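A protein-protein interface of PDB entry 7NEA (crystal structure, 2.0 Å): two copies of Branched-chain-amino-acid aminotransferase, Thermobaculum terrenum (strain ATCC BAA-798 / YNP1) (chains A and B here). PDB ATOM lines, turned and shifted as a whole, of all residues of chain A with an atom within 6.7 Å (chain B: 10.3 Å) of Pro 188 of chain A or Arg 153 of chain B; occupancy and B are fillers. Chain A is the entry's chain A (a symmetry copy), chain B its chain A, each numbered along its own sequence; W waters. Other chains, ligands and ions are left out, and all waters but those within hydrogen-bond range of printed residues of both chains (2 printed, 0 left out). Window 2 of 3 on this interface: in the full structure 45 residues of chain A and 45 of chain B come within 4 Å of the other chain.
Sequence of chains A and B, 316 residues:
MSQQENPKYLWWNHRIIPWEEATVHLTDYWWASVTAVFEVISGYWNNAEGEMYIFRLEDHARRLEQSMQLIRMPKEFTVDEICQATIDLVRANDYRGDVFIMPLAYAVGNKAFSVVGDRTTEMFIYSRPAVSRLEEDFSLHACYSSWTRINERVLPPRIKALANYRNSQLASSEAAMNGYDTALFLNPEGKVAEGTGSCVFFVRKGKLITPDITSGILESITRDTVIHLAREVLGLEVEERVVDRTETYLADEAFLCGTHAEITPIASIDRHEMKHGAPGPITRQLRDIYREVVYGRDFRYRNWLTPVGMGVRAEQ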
ATOM      1  N   SER A 146      39.552  -6.335 -24.384  1.00  0.00           N
ATOM      2  CA  SER A 146      39.052  -7.340 -23.432  1.00  0.00           C
ATOM      3  C   SER A 146      37.538  -7.548 -23.533  1.00  0.00           C
ATOM      4  O   SER A 146      37.026  -8.408 -22.758  1.00  0.00           O
ATOM      5  CB  SER A 146      39.400  -6.954 -22.054  1.00  0.00           C
ATOM      6  OG  SER A 146      38.769  -5.749 -21.725  1.00  0.00           O
ATOM      7  N   TRP A 147      36.847  -6.732 -24.341  1.00  0.00           N
ATOM      8  CA  TRP A 147      35.418  -6.923 -24.620  1.00  0.00           C
ATOM      9  C   TRP A 147      35.262  -7.720 -25.911  1.00  0.00           C
ATOM     10  O   TRP A 147      36.010  -7.442 -26.881  1.00  0.00           O
ATOM     11  CB  TRP A 147      34.730  -5.567 -24.674  1.00  0.00           C
ATOM     12  CG  TRP A 147      34.854  -4.816 -23.397  1.00  0.00           C
ATOM     13  CD1 TRP A 147      35.745  -3.844 -23.067  1.00  0.00           C
ATOM     14  CD2 TRP A 147      33.986  -4.971 -22.283  1.00  0.00           C
ATOM     15  NE1 TRP A 147      35.516  -3.425 -21.782  1.00  0.00           N
ATOM     16  CE2 TRP A 147      34.445  -4.099 -21.276  1.00  0.00           C
ATOM     17  CE3 TRP A 147      32.872  -5.784 -22.048  1.00  0.00           C
ATOM     18  CZ2 TRP A 147      33.793  -3.977 -20.046  1.00  0.00           C
ATOM     19  CZ3 TRP A 147      32.227  -5.679 -20.833  1.00  0.00           C
ATOM     20  CH2 TRP A 147      32.674  -4.760 -19.860  1.00  0.00           C
ATOM     21  N   THR A 148      34.270  -8.616 -25.916  1.00  0.00           N
ATOM     22  CA  THR A 148      34.008  -9.583 -26.998  1.00  0.00           C
ATOM     23  C   THR A 148      33.080  -8.942 -28.041  1.00  0.00           C
ATOM     24  O   THR A 148      32.157  -8.237 -27.652  1.00  0.00           O
ATOM     25  CB  THR A 148      33.432 -10.881 -26.426  1.00  0.00           C
ATOM     26  OG1 THR A 148      34.316 -11.339 -25.382  1.00  0.00           O
ATOM     27  CG2 THR A 148      33.261 -11.941 -27.500  1.00  0.00           C
ATOM     28  N   ARG A 149      33.233  -9.299 -29.309  1.00  0.00           N
ATOM     29  CA  ARG A 149      32.336  -8.789 -30.361  1.00  0.00           C
ATOM     30  C   ARG A 149      30.989  -9.548 -30.295  1.00  0.00           C
ATOM     31  O   ARG A 149      30.961 -10.765 -30.058  1.00  0.00           O
ATOM     32  CB  ARG A 149      32.965  -8.979 -31.742  1.00  0.00           C
ATOM     33  CG  ARG A 149      32.221  -8.282 -32.890  1.00  0.00           C
ATOM     34  CD  ARG A 149      32.087  -6.782 -32.646  1.00  0.00           C
ATOM     35  NE  ARG A 149      31.407  -6.073 -33.722  1.00  0.00           N
ATOM     36  CZ  ARG A 149      30.849  -4.841 -33.669  1.00  0.00           C
ATOM     37  NH1 ARG A 149      30.719  -4.143 -32.540  1.00  0.00           N
ATOM     38  NH2 ARG A 149      30.359  -4.317 -34.791  1.00  0.00           N
ATOM     39  N   ILE A 150      29.895  -8.816 -30.466  1.00  0.00           N
ATOM     40  CA  ILE A 150      28.520  -9.366 -30.695  1.00  0.00           C
ATOM     41  C   ILE A 150      28.587 -10.421 -31.797  1.00  0.00           C
ATOM     42  O   ILE A 150      29.407 -10.304 -32.730  1.00  0.00           O
ATOM     43  CB  ILE A 150      27.528  -8.242 -31.100  1.00  0.00           C
ATOM     44  CG1 ILE A 150      28.142  -7.361 -32.215  1.00  0.00           C
ATOM     45  CG2 ILE A 150      27.119  -7.450 -29.887  1.00  0.00           C
ATOM     46  CD1 ILE A 150      27.204  -6.404 -32.848  1.00  0.00           C
ATOM     47  N   ASN A 151      27.729 -11.427 -31.715  1.00  0.00           N
ATOM     48  CA  ASN A 151      27.657 -12.488 -32.748  1.00  0.00           C
ATOM     49  C   ASN A 151      26.193 -12.662 -33.178  1.00  0.00           C
ATOM     50  O   ASN A 151      25.280 -11.959 -32.597  1.00  0.00           O
ATOM     51  CB  ASN A 151      28.263 -13.794 -32.217  1.00  0.00           C
ATOM     52  CG  ASN A 151      27.523 -14.362 -31.012  1.00  0.00           C
ATOM     53  OD1 ASN A 151      26.672 -13.700 -30.428  1.00  0.00           O
ATOM     54  ND2 ASN A 151      27.936 -15.538 -30.556  1.00  0.00           N
ATOM     55  N   ASN A 167      28.334  -2.026 -28.256  1.00  0.00           N
ATOM     56  CA  ASN A 167      29.437  -3.025 -28.107  1.00  0.00           C
ATOM     57  C   ASN A 167      30.751  -2.383 -28.624  1.00  0.00           C
ATOM     58  O   ASN A 167      31.791  -2.485 -27.947  1.00  0.00           O
ATOM     59  CB  ASN A 167      29.099  -4.283 -28.902  1.00  0.00           C
ATOM     60  CG  ASN A 167      30.215  -5.307 -28.929  1.00  0.00           C
ATOM     61  OD1 ASN A 167      30.791  -5.574 -29.987  1.00  0.00           O
ATOM     62  ND2 ASN A 167      30.454  -5.943 -27.795  1.00  0.00           N
ATOM     63  N   LEU A 170      32.401  -0.098 -25.994  1.00  0.00           N
ATOM     64  CA  LEU A 170      33.138  -0.812 -24.906  1.00  0.00           C
ATOM     65  C   LEU A 170      34.631  -0.900 -25.307  1.00  0.00           C
ATOM     66  O   LEU A 170      35.525  -0.620 -24.488  1.00  0.00           O
ATOM     67  CB  LEU A 170      32.558  -2.222 -24.690  1.00  0.00           C
ATOM     68  CG  LEU A 170      31.176  -2.273 -24.070  1.00  0.00           C
ATOM     69  CD1 LEU A 170      30.578  -3.690 -24.219  1.00  0.00           C
ATOM     70  CD2 LEU A 170      31.215  -1.835 -22.588  1.00  0.00           C
ATOM     71  N   LEU A 186      38.011  -9.628 -30.916  1.00  0.00           N
ATOM     72  CA  LEU A 186      37.869 -11.095 -31.038  1.00  0.00           C
ATOM     73  C   LEU A 186      36.403 -11.488 -30.917  1.00  0.00           C
ATOM     74  O   LEU A 186      35.643 -10.747 -30.206  1.00  0.00           O
ATOM     75  CB  LEU A 186      38.630 -11.675 -29.876  1.00  0.00           C
ATOM     76  CG  LEU A 186      40.058 -11.216 -29.800  1.00  0.00           C
ATOM     77  CD1 LEU A 186      40.608 -11.846 -28.561  1.00  0.00           C
ATOM     78  CD2 LEU A 186      40.832 -11.615 -31.055  1.00  0.00           C
ATOM     79  N   ASN A 187      36.022 -12.586 -31.591  1.00  0.00           N
ATOM     80  CA  ASN A 187      34.621 -13.054 -31.535  1.00  0.00           C
ATOM     81  C   ASN A 187      34.510 -13.949 -30.315  1.00  0.00           C
ATOM     82  O   ASN A 187      35.515 -14.198 -29.643  1.00  0.00           O
ATOM     83  CB  ASN A 187      34.142 -13.659 -32.848  1.00  0.00           C
ATOM     84  CG  ASN A 187      34.810 -14.968 -33.174  1.00  0.00           C
ATOM     85  OD1 ASN A 187      35.475 -15.568 -32.318  1.00  0.00           O
ATOM     86  ND2 ASN A 187      34.705 -15.333 -34.457  1.00  0.00           N
ATOM     87  N   PRO A 188      33.294 -14.423 -29.967  1.00  0.00           N
ATOM     88  CA  PRO A 188      33.139 -15.285 -28.776  1.00  0.00           C
ATOM     89  C   PRO A 188      33.994 -16.557 -28.725  1.00  0.00           C
ATOM     90  O   PRO A 188      34.407 -16.961 -27.603  1.00  0.00           O
ATOM     91  CB  PRO A 188      31.624 -15.578 -28.788  1.00  0.00           C
ATOM     92  CG  PRO A 188      31.033 -14.337 -29.427  1.00  0.00           C
ATOM     93  CD  PRO A 188      31.994 -13.992 -30.556  1.00  0.00           C
ATOM     94  N   GLU A 189      34.290 -17.142 -29.905  1.00  0.00           N
ATOM     95  CA  GLU A 189      35.181 -18.314 -30.010  1.00  0.00           C
ATOM     96  C   GLU A 189      36.655 -17.866 -29.883  1.00  0.00           C
ATOM     97  O   GLU A 189      37.493 -18.745 -29.910  1.00  0.00           O
ATOM     98  CB  GLU A 189      34.849 -19.084 -31.302  1.00  0.00           C
ATOM     99  CG  GLU A 189      33.527 -19.864 -31.214  1.00  0.00           C
ATOM    100  CD  GLU A 189      32.293 -18.963 -31.136  1.00  0.00           C
ATOM    101  OE1 GLU A 189      32.155 -17.997 -32.013  1.00  0.00           O
ATOM    102  OE2 GLU A 189      31.464 -19.203 -30.229  1.00  0.00           O
ATOM    103  N   GLY A 190      36.975 -16.563 -29.866  1.00  0.00           N
ATOM    104  CA  GLY A 190      38.377 -16.133 -29.685  1.00  0.00           C
ATOM    105  C   GLY A 190      39.068 -15.812 -31.008  1.00  0.00           C
ATOM    106  O   GLY A 190      40.306 -15.593 -30.991  1.00  0.00           O
ATOM    107  N   LYS A 191      38.342 -15.795 -32.140  1.00  0.00           N
ATOM    108  CA  LYS A 191      38.985 -15.588 -33.493  1.00  0.00           C
ATOM    109  C   LYS A 191      38.872 -14.083 -33.846  1.00  0.00           C
ATOM    110  O   LYS A 191      38.013 -13.409 -33.280  1.00  0.00           O
ATOM    111  CB  LYS A 191      38.346 -16.466 -34.586  1.00  0.00           C
ATOM    112  CG  LYS A 191      38.330 -17.979 -34.289  1.00  0.00           C
ATOM    113  CD  LYS A 191      39.710 -18.505 -33.855  1.00  0.00           C
ATOM    114  CE  LYS A 191      39.719 -20.021 -33.601  1.00  0.00           C
ATOM    115  NZ  LYS A 191      40.997 -20.478 -33.009  1.00  0.00           N
ATOM    116  N   SER A 215      33.000 -14.954 -39.540  1.00  0.00           N
ATOM    117  CA  SER A 215      33.788 -14.651 -38.301  1.00  0.00           C
ATOM    118  C   SER A 215      33.030 -13.671 -37.407  1.00  0.00           C
ATOM    119  O   SER A 215      33.438 -13.480 -36.223  1.00  0.00           O
ATOM    120  CB  SER A 215      35.169 -14.079 -38.635  1.00  0.00           C
ATOM    121  OG  SER A 215      35.982 -15.019 -39.290  1.00  0.00           O
ATOM    122  N   THR B 148      19.311 -15.442 -28.398  1.00  0.00           N
ATOM    123  CA  THR B 148      20.048 -15.583 -27.129  1.00  0.00           C
ATOM    124  C   THR B 148      20.117 -14.220 -26.425  1.00  0.00           C
ATOM    125  O   THR B 148      20.309 -13.217 -27.102  1.00  0.00           O
ATOM    126  CB  THR B 148      21.435 -16.181 -27.381  1.00  0.00           C
ATOM    127  OG1 THR B 148      21.267 -17.394 -28.143  1.00  0.00           O
ATOM    128  CG2 THR B 148      22.174 -16.449 -26.083  1.00  0.00           C
ATOM    129  N   ARG B 149      20.111 -14.207 -25.099  1.00  0.00           N
ATOM    130  CA  ARG B 149      20.251 -12.948 -24.345  1.00  0.00           C
ATOM    131  C   ARG B 149      21.734 -12.508 -24.357  1.00  0.00           C
ATOM    132  O   ARG B 149      22.642 -13.346 -24.248  1.00  0.00           O
ATOM    133  CB  ARG B 149      19.781 -13.131 -22.901  1.00  0.00           C
ATOM    134  CG  ARG B 149      19.671 -11.832 -22.090  1.00  0.00           C
ATOM    135  CD  ARG B 149      18.733 -10.831 -22.757  1.00  0.00           C
ATOM    136  NE  ARG B 149      18.577  -9.589 -22.011  1.00  0.00           N
ATOM    137  CZ  ARG B 149      18.102  -8.408 -22.472  1.00  0.00           C
ATOM    138  NH1 ARG B 149      17.834  -8.177 -23.757  1.00  0.00           N
ATOM    139  NH2 ARG B 149      17.940  -7.409 -21.607  1.00  0.00           N
ATOM    140  N   ILE B 150      21.959 -11.211 -24.529  1.00  0.00           N
ATOM    141  CA  ILE B 150      23.279 -10.533 -24.322  1.00  0.00           C
ATOM    142  C   ILE B 150      23.848 -10.960 -22.970  1.00  0.00           C
ATOM    143  O   ILE B 150      23.081 -11.203 -22.015  1.00  0.00           O
ATOM    144  CB  ILE B 150      23.129  -8.988 -24.367  1.00  0.00           C
ATOM    145  CG1 ILE B 150      21.945  -8.538 -23.478  1.00  0.00           C
ATOM    146  CG2 ILE B 150      22.999  -8.523 -25.793  1.00  0.00           C
ATOM    147  CD1 ILE B 150      21.847  -7.077 -23.253  1.00  0.00           C
ATOM    148  N   ASN B 151      25.166 -11.030 -22.870  1.00  0.00           N
ATOM    149  CA  ASN B 151      25.843 -11.381 -21.599  1.00  0.00           C
ATOM    150  C   ASN B 151      26.936 -10.339 -21.315  1.00  0.00           C
ATOM    151  O   ASN B 151      27.144  -9.400 -22.173  1.00  0.00           O
ATOM    152  CB  ASN B 151      26.407 -12.807 -21.668  1.00  0.00           C
ATOM    153  CG  ASN B 151      27.468 -12.989 -22.746  1.00  0.00           C
ATOM    154  OD1 ASN B 151      27.664 -12.120 -23.588  1.00  0.00           O
ATOM    155  ND2 ASN B 151      28.065 -14.173 -22.803  1.00  0.00           N
ATOM    156  N   GLU B 152      27.674 -10.510 -20.207  1.00  0.00           N
ATOM    157  CA  GLU B 152      28.739  -9.533 -19.820  1.00  0.00           C
ATOM    158  C   GLU B 152      29.858  -9.533 -20.870  1.00  0.00           C
ATOM    159  O   GLU B 152      30.639  -8.536 -20.953  1.00  0.00           O
ATOM    160  CB  GLU B 152      29.253  -9.893 -18.424  1.00  0.00           C
ATOM    161  CG  GLU B 152      28.273  -9.401 -17.368  1.00  0.00           C
ATOM    162  CD  GLU B 152      28.641  -8.131 -16.610  1.00  0.00           C
ATOM    163  OE1 GLU B 152      29.824  -7.808 -16.501  1.00  0.00           O
ATOM    164  OE2 GLU B 152      27.740  -7.537 -16.051  1.00  0.00           O
ATOM    165  N   ARG B 153      30.003 -10.616 -21.616  1.00  0.00           N
ATOM    166  CA  ARG B 153      31.106 -10.701 -22.589  1.00  0.00           C
ATOM    167  C   ARG B 153      30.968  -9.589 -23.641  1.00  0.00           C
ATOM    168  O   ARG B 153      32.021  -9.047 -24.071  1.00  0.00           O
ATOM    169  CB  ARG B 153      31.088 -12.095 -23.225  1.00  0.00           C
ATOM    170  CG  ARG B 153      31.519 -13.235 -22.305  1.00  0.00           C
ATOM    171  CD  ARG B 153      32.003 -14.476 -23.034  1.00  0.00           C
ATOM    172  NE  ARG B 153      33.230 -14.219 -23.793  1.00  0.00           N
ATOM    173  CZ  ARG B 153      33.687 -14.964 -24.805  1.00  0.00           C
ATOM    174  NH1 ARG B 153      34.758 -14.567 -25.446  1.00  0.00           N
ATOM    175  NH2 ARG B 153      33.047 -16.061 -25.226  1.00  0.00           N
ATOM    176  N   VAL B 154      29.725  -9.266 -24.068  1.00  0.00           N
ATOM    177  CA  VAL B 154      29.430  -8.404 -25.258  1.00  0.00           C
ATOM    178  C   VAL B 154      28.617  -7.169 -24.874  1.00  0.00           C
ATOM    179  O   VAL B 154      28.852  -6.129 -25.512  1.00  0.00           O
ATOM    180  CB  VAL B 154      28.719  -9.224 -26.366  1.00  0.00           C
ATOM    181  CG1 VAL B 154      29.552 -10.473 -26.787  1.00  0.00           C
ATOM    182  CG2 VAL B 154      27.298  -9.615 -25.995  1.00  0.00           C
ATOM    183  N   LEU B 155      27.629  -7.254 -23.978  1.00  0.00           N
ATOM    184  CA  LEU B 155      26.759  -6.068 -23.675  1.00  0.00           C
ATOM    185  C   LEU B 155      26.160  -6.280 -22.278  1.00  0.00           C
ATOM    186  O   LEU B 155      25.079  -6.877 -22.131  1.00  0.00           O
ATOM    187  CB  LEU B 155      25.594  -5.954 -24.673  1.00  0.00           C
ATOM    188  CG  LEU B 155      25.685  -5.142 -25.979  1.00  0.00           C
ATOM    189  CD1 LEU B 155      24.271  -4.764 -26.445  1.00  0.00           C
ATOM    190  CD2 LEU B 155      26.516  -3.892 -25.874  1.00  0.00           C
ATOM    191  N   PRO B 156      26.863  -5.869 -21.203  1.00  0.00           N
ATOM    192  CA  PRO B 156      26.414  -6.237 -19.853  1.00  0.00           C
ATOM    193  C   PRO B 156      24.955  -5.857 -19.633  1.00  0.00           C
ATOM    194  O   PRO B 156      24.537  -4.672 -19.706  1.00  0.00           O
ATOM    195  CB  PRO B 156      27.416  -5.472 -18.975  1.00  0.00           C
ATOM    196  CG  PRO B 156      28.688  -5.466 -19.821  1.00  0.00           C
ATOM    197  CD  PRO B 156      28.146  -5.148 -21.202  1.00  0.00           C
ATOM    198  N   PRO B 157      24.132  -6.854 -19.329  1.00  0.00           N
ATOM    199  CA  PRO B 157      22.747  -6.583 -18.981  1.00  0.00           C
ATOM    200  C   PRO B 157      22.572  -5.758 -17.715  1.00  0.00           C
ATOM    201  O   PRO B 157      21.542  -5.214 -17.524  1.00  0.00           O
ATOM    202  CB  PRO B 157      22.134  -7.973 -18.744  1.00  0.00           C
ATOM    203  CG  PRO B 157      23.102  -8.966 -19.255  1.00  0.00           C
ATOM    204  CD  PRO B 157      24.457  -8.300 -19.326  1.00  0.00           C
ATOM    205  N   ARG B 158      23.581  -5.650 -16.856  1.00  0.00           N
ATOM    206  CA  ARG B 158      23.471  -4.798 -15.631  1.00  0.00           C
ATOM    207  C   ARG B 158      23.218  -3.338 -16.045  1.00  0.00           C
ATOM    208  O   ARG B 158      22.674  -2.569 -15.224  1.00  0.00           O
ATOM    209  CB  ARG B 158      24.794  -4.847 -14.851  1.00  0.00           C
ATOM    210  CG  ARG B 158      24.971  -3.715 -13.855  1.00  0.00           C
ATOM    211  CD  ARG B 158      26.108  -3.948 -12.849  1.00  0.00           C
ATOM    212  NE  ARG B 158      25.926  -5.151 -12.072  1.00  0.00           N
ATOM    213  CZ  ARG B 158      25.097  -5.315 -11.040  1.00  0.00           C
ATOM    214  NH1 ARG B 158      24.332  -4.330 -10.554  1.00  0.00           N
ATOM    215  NH2 ARG B 158      25.041  -6.518 -10.503  1.00  0.00           N
ATOM    216  N   ILE B 159      23.740  -2.903 -17.217  1.00  0.00           N
ATOM    217  CA  ILE B 159      23.644  -1.475 -17.685  1.00  0.00           C
ATOM    218  C   ILE B 159      22.274  -1.325 -18.305  1.00  0.00           C
ATOM    219  O   ILE B 159      21.947  -2.078 -19.249  1.00  0.00           O
ATOM    220  CB  ILE B 159      24.741  -1.081 -18.691  1.00  0.00           C
ATOM    221  CG1 ILE B 159      26.135  -1.400 -18.164  1.00  0.00           C
ATOM    222  CG2 ILE B 159      24.559   0.384 -19.081  1.00  0.00           C
ATOM    223  CD1 ILE B 159      27.324  -1.285 -19.200  1.00  0.00           C
ATOM    224  N   ASN B 187      20.217 -17.680 -21.675  1.00  0.00           N
ATOM    225  CA  ASN B 187      21.532 -17.009 -21.765  1.00  0.00           C
ATOM    226  C   ASN B 187      22.387 -17.854 -22.691  1.00  0.00           C
ATOM    227  O   ASN B 187      21.943 -18.913 -23.142  1.00  0.00           O
ATOM    228  CB  ASN B 187      22.137 -16.698 -20.402  1.00  0.00           C
ATOM    229  CG  ASN B 187      22.557 -17.931 -19.647  1.00  0.00           C
ATOM    230  OD1 ASN B 187      22.620 -19.029 -20.215  1.00  0.00           O
ATOM    231  ND2 ASN B 187      22.735 -17.735 -18.335  1.00  0.00           N
ATOM    232  N   PRO B 188      23.612 -17.398 -23.035  1.00  0.00           N
ATOM    233  CA  PRO B 188      24.471 -18.182 -23.949  1.00  0.00           C
ATOM    234  C   PRO B 188      24.780 -19.627 -23.540  1.00  0.00           C
ATOM    235  O   PRO B 188      24.912 -20.494 -24.447  1.00  0.00           O
ATOM    236  CB  PRO B 188      25.733 -17.299 -24.036  1.00  0.00           C
ATOM    237  CG  PRO B 188      25.192 -15.895 -23.845  1.00  0.00           C
ATOM    238  CD  PRO B 188      24.143 -16.035 -22.749  1.00  0.00           C
ATOM    239  N   GLU B 189      24.847 -19.888 -22.218  1.00  0.00           N
ATOM    240  CA  GLU B 189      25.041 -21.251 -21.685  1.00  0.00           C
ATOM    241  C   GLU B 189      23.711 -22.037 -21.754  1.00  0.00           C
ATOM    242  O   GLU B 189      23.745 -23.192 -21.384  1.00  0.00           O
ATOM    243  CB  GLU B 189      25.663 -21.157 -20.278  1.00  0.00           C
ATOM    244  CG  GLU B 189      27.146 -20.754 -20.303  1.00  0.00           C
ATOM    245  CD  GLU B 189      27.379 -19.317 -20.776  1.00  0.00           C
ATOM    246  OE1 GLU B 189      26.687 -18.348 -20.225  1.00  0.00           O
ATOM    247  OE2 GLU B 189      28.235 -19.140 -21.671  1.00  0.00           O
ATOM    248  N   THR B 214      23.752 -13.237 -11.710  1.00  0.00           N
ATOM    249  CA  THR B 214      24.874 -13.610 -12.637  1.00  0.00           C
ATOM    250  C   THR B 214      24.358 -14.579 -13.726  1.00  0.00           C
ATOM    251  O   THR B 214      25.195 -15.016 -14.556  1.00  0.00           O
ATOM    252  CB  THR B 214      26.084 -14.155 -11.842  1.00  0.00           C
ATOM    253  OG1 THR B 214      25.633 -15.240 -11.020  1.00  0.00           O
ATOM    254  CG2 THR B 214      26.723 -13.091 -10.971  1.00  0.00           C
ATOM    255  N   SER B 215      23.048 -14.867 -13.801  1.00  0.00           N
ATOM    256  CA  SER B 215      22.434 -15.572 -14.972  1.00  0.00           C
ATOM    257  C   SER B 215      22.376 -14.649 -16.187  1.00  0.00           C
ATOM    258  O   SER B 215      22.098 -15.143 -17.320  1.00  0.00           O
ATOM    259  CB  SER B 215      21.027 -16.084 -14.648  1.00  0.00           C
ATOM    260  OG  SER B 215      21.046 -17.086 -13.665  1.00  0.00           O
ATOM    261  N   GLY B 216      22.687 -13.361 -15.969  1.00  0.00           N
ATOM    262  CA  GLY B 216      22.813 -12.303 -16.971  1.00  0.00           C
ATOM    263  C   GLY B 216      21.508 -11.563 -17.187  1.00  0.00           C
ATOM    264  O   GLY B 216      20.853 -11.685 -18.259  1.00  0.00           O
HETATM  265  O   HOH W   1      34.856  -9.992 -22.827  1.00  0.00           O
HETATM  266  O   HOH W   2      36.837 -13.675 -27.272  1.00  0.00           O
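N of Thr 148 of chain A lies within hydrogen-bond range of O of Arg 153 of chain B (2.9 Å). The guanidinium group (NH2) of Arg 153 of chain B sits at hydrogen-bond distance from the backbone carbonyl oxygen (O) of Pro 188 of chain A. The backbone carbonyl oxygen (O) of Val 154 of chain B sits at hydrogen-bond distance from the side-chain amide nitrogen (ND2) of Asn 167 of chain A.
Of the printed residues of chain B, Trp 147 of chain A touches Glu 152 (3.3 Å), Arg 153 (3.9 Å) and Pro 156 (3.7 Å). Thr 148 of chain A touches two residues of chain B. Of the printed residues of chain B, Arg 149 of chain A touches Val 154. Of the printed residues of chain B, Asn 167 of chain A touches Val 154 and Leu 155. No residue of chain B comes within 4 Å of Asn 187 of chain A. Of chain B, only Arg 153 comes within 4 Å of Pro 188 of chain A. Printed residues of chain A within 4 Å of Glu 152 of chain B: Trp 147. Of the printed residues of chain A, Leu 155 of chain B touches Asn 167 (3.5 Å). The nearest residue of chain B that does not touch Pro 188 of chain A is Val 154 of chain B (4.9 Å). The nearest printed residue of chain B that does not touch Leu 170 of chain A is Pro 156 of chain B (4.1 Å).
Positions printed for both chains: 148, 149, 150, 151, 187, 188, 189 and 215.
Glu 152 of chain B touches Trp 147 of chain A (O to CZ3, 3.3 Å). Trp 147 of chain A touches Arg 153 of chain B. CZ3 of Trp 147 of chain A touches CG of Pro 156 of chain B, 3.7 Å away. Thr 148 of chain A touches Val 154 of chain B (O to CG1, 3.5 Å). O of Arg 149 of chain A touches CG1 of Val 154 of chain B (3.6 Å). Leu 155 of chain B touches Asn 167 of chain A (CD2 to N, 3.5 Å). Val 154 of chain B touches Leu 170 of chain A.
Along chain A the printed residues that touch a printed residue of chain B span positions 147 to 188. Of the 18 printed residues of chain B, 5 touch a printed residue of chain A. Hydrophobic or aromatic side chains of chain B within 4 Å of the printed part of chain A: Val 154, Leu 155 and Pro 156.
The backbone NH of Arg 153 of chain B lies close to the side-chain amide oxygen of Asn 151 of chain B, 3.4 Å away. O of Thr 148 of chain A lies within hydrogen-bond range of ND2 of Asn 167 of chain A (2.9 Å). The guanidinium group of Arg 149 of chain A lies within hydrogen-bond range of the side-chain amide oxygen of Asn 167 of chain A (2.9 Å). The backbone carbonyl oxygen (O) of Leu 186 of chain A lies within hydrogen-bond range of the backbone NH (N) of Arg 149 of chain A. The backbone NH (N) of Ile 150 of chain A is in hydrogen-bond range of the side-chain amide oxygen (OD1) of Asn 167 of chain A (3.4 Å).
Water W1 lies within hydrogen-bond range of O of Ser 146 of chain A (2.7 Å), OG1 of Thr 148 of chain A (2.9 Å) and O of Arg 153 of chain B (3.2 Å). Water W2 lies within hydrogen-bond range of the backbone carbonyl oxygen (O) of Asn 187 of chain A (2.8 Å) and the guanidinium group (NH1) of Arg 153 of chain B (2.9 Å).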
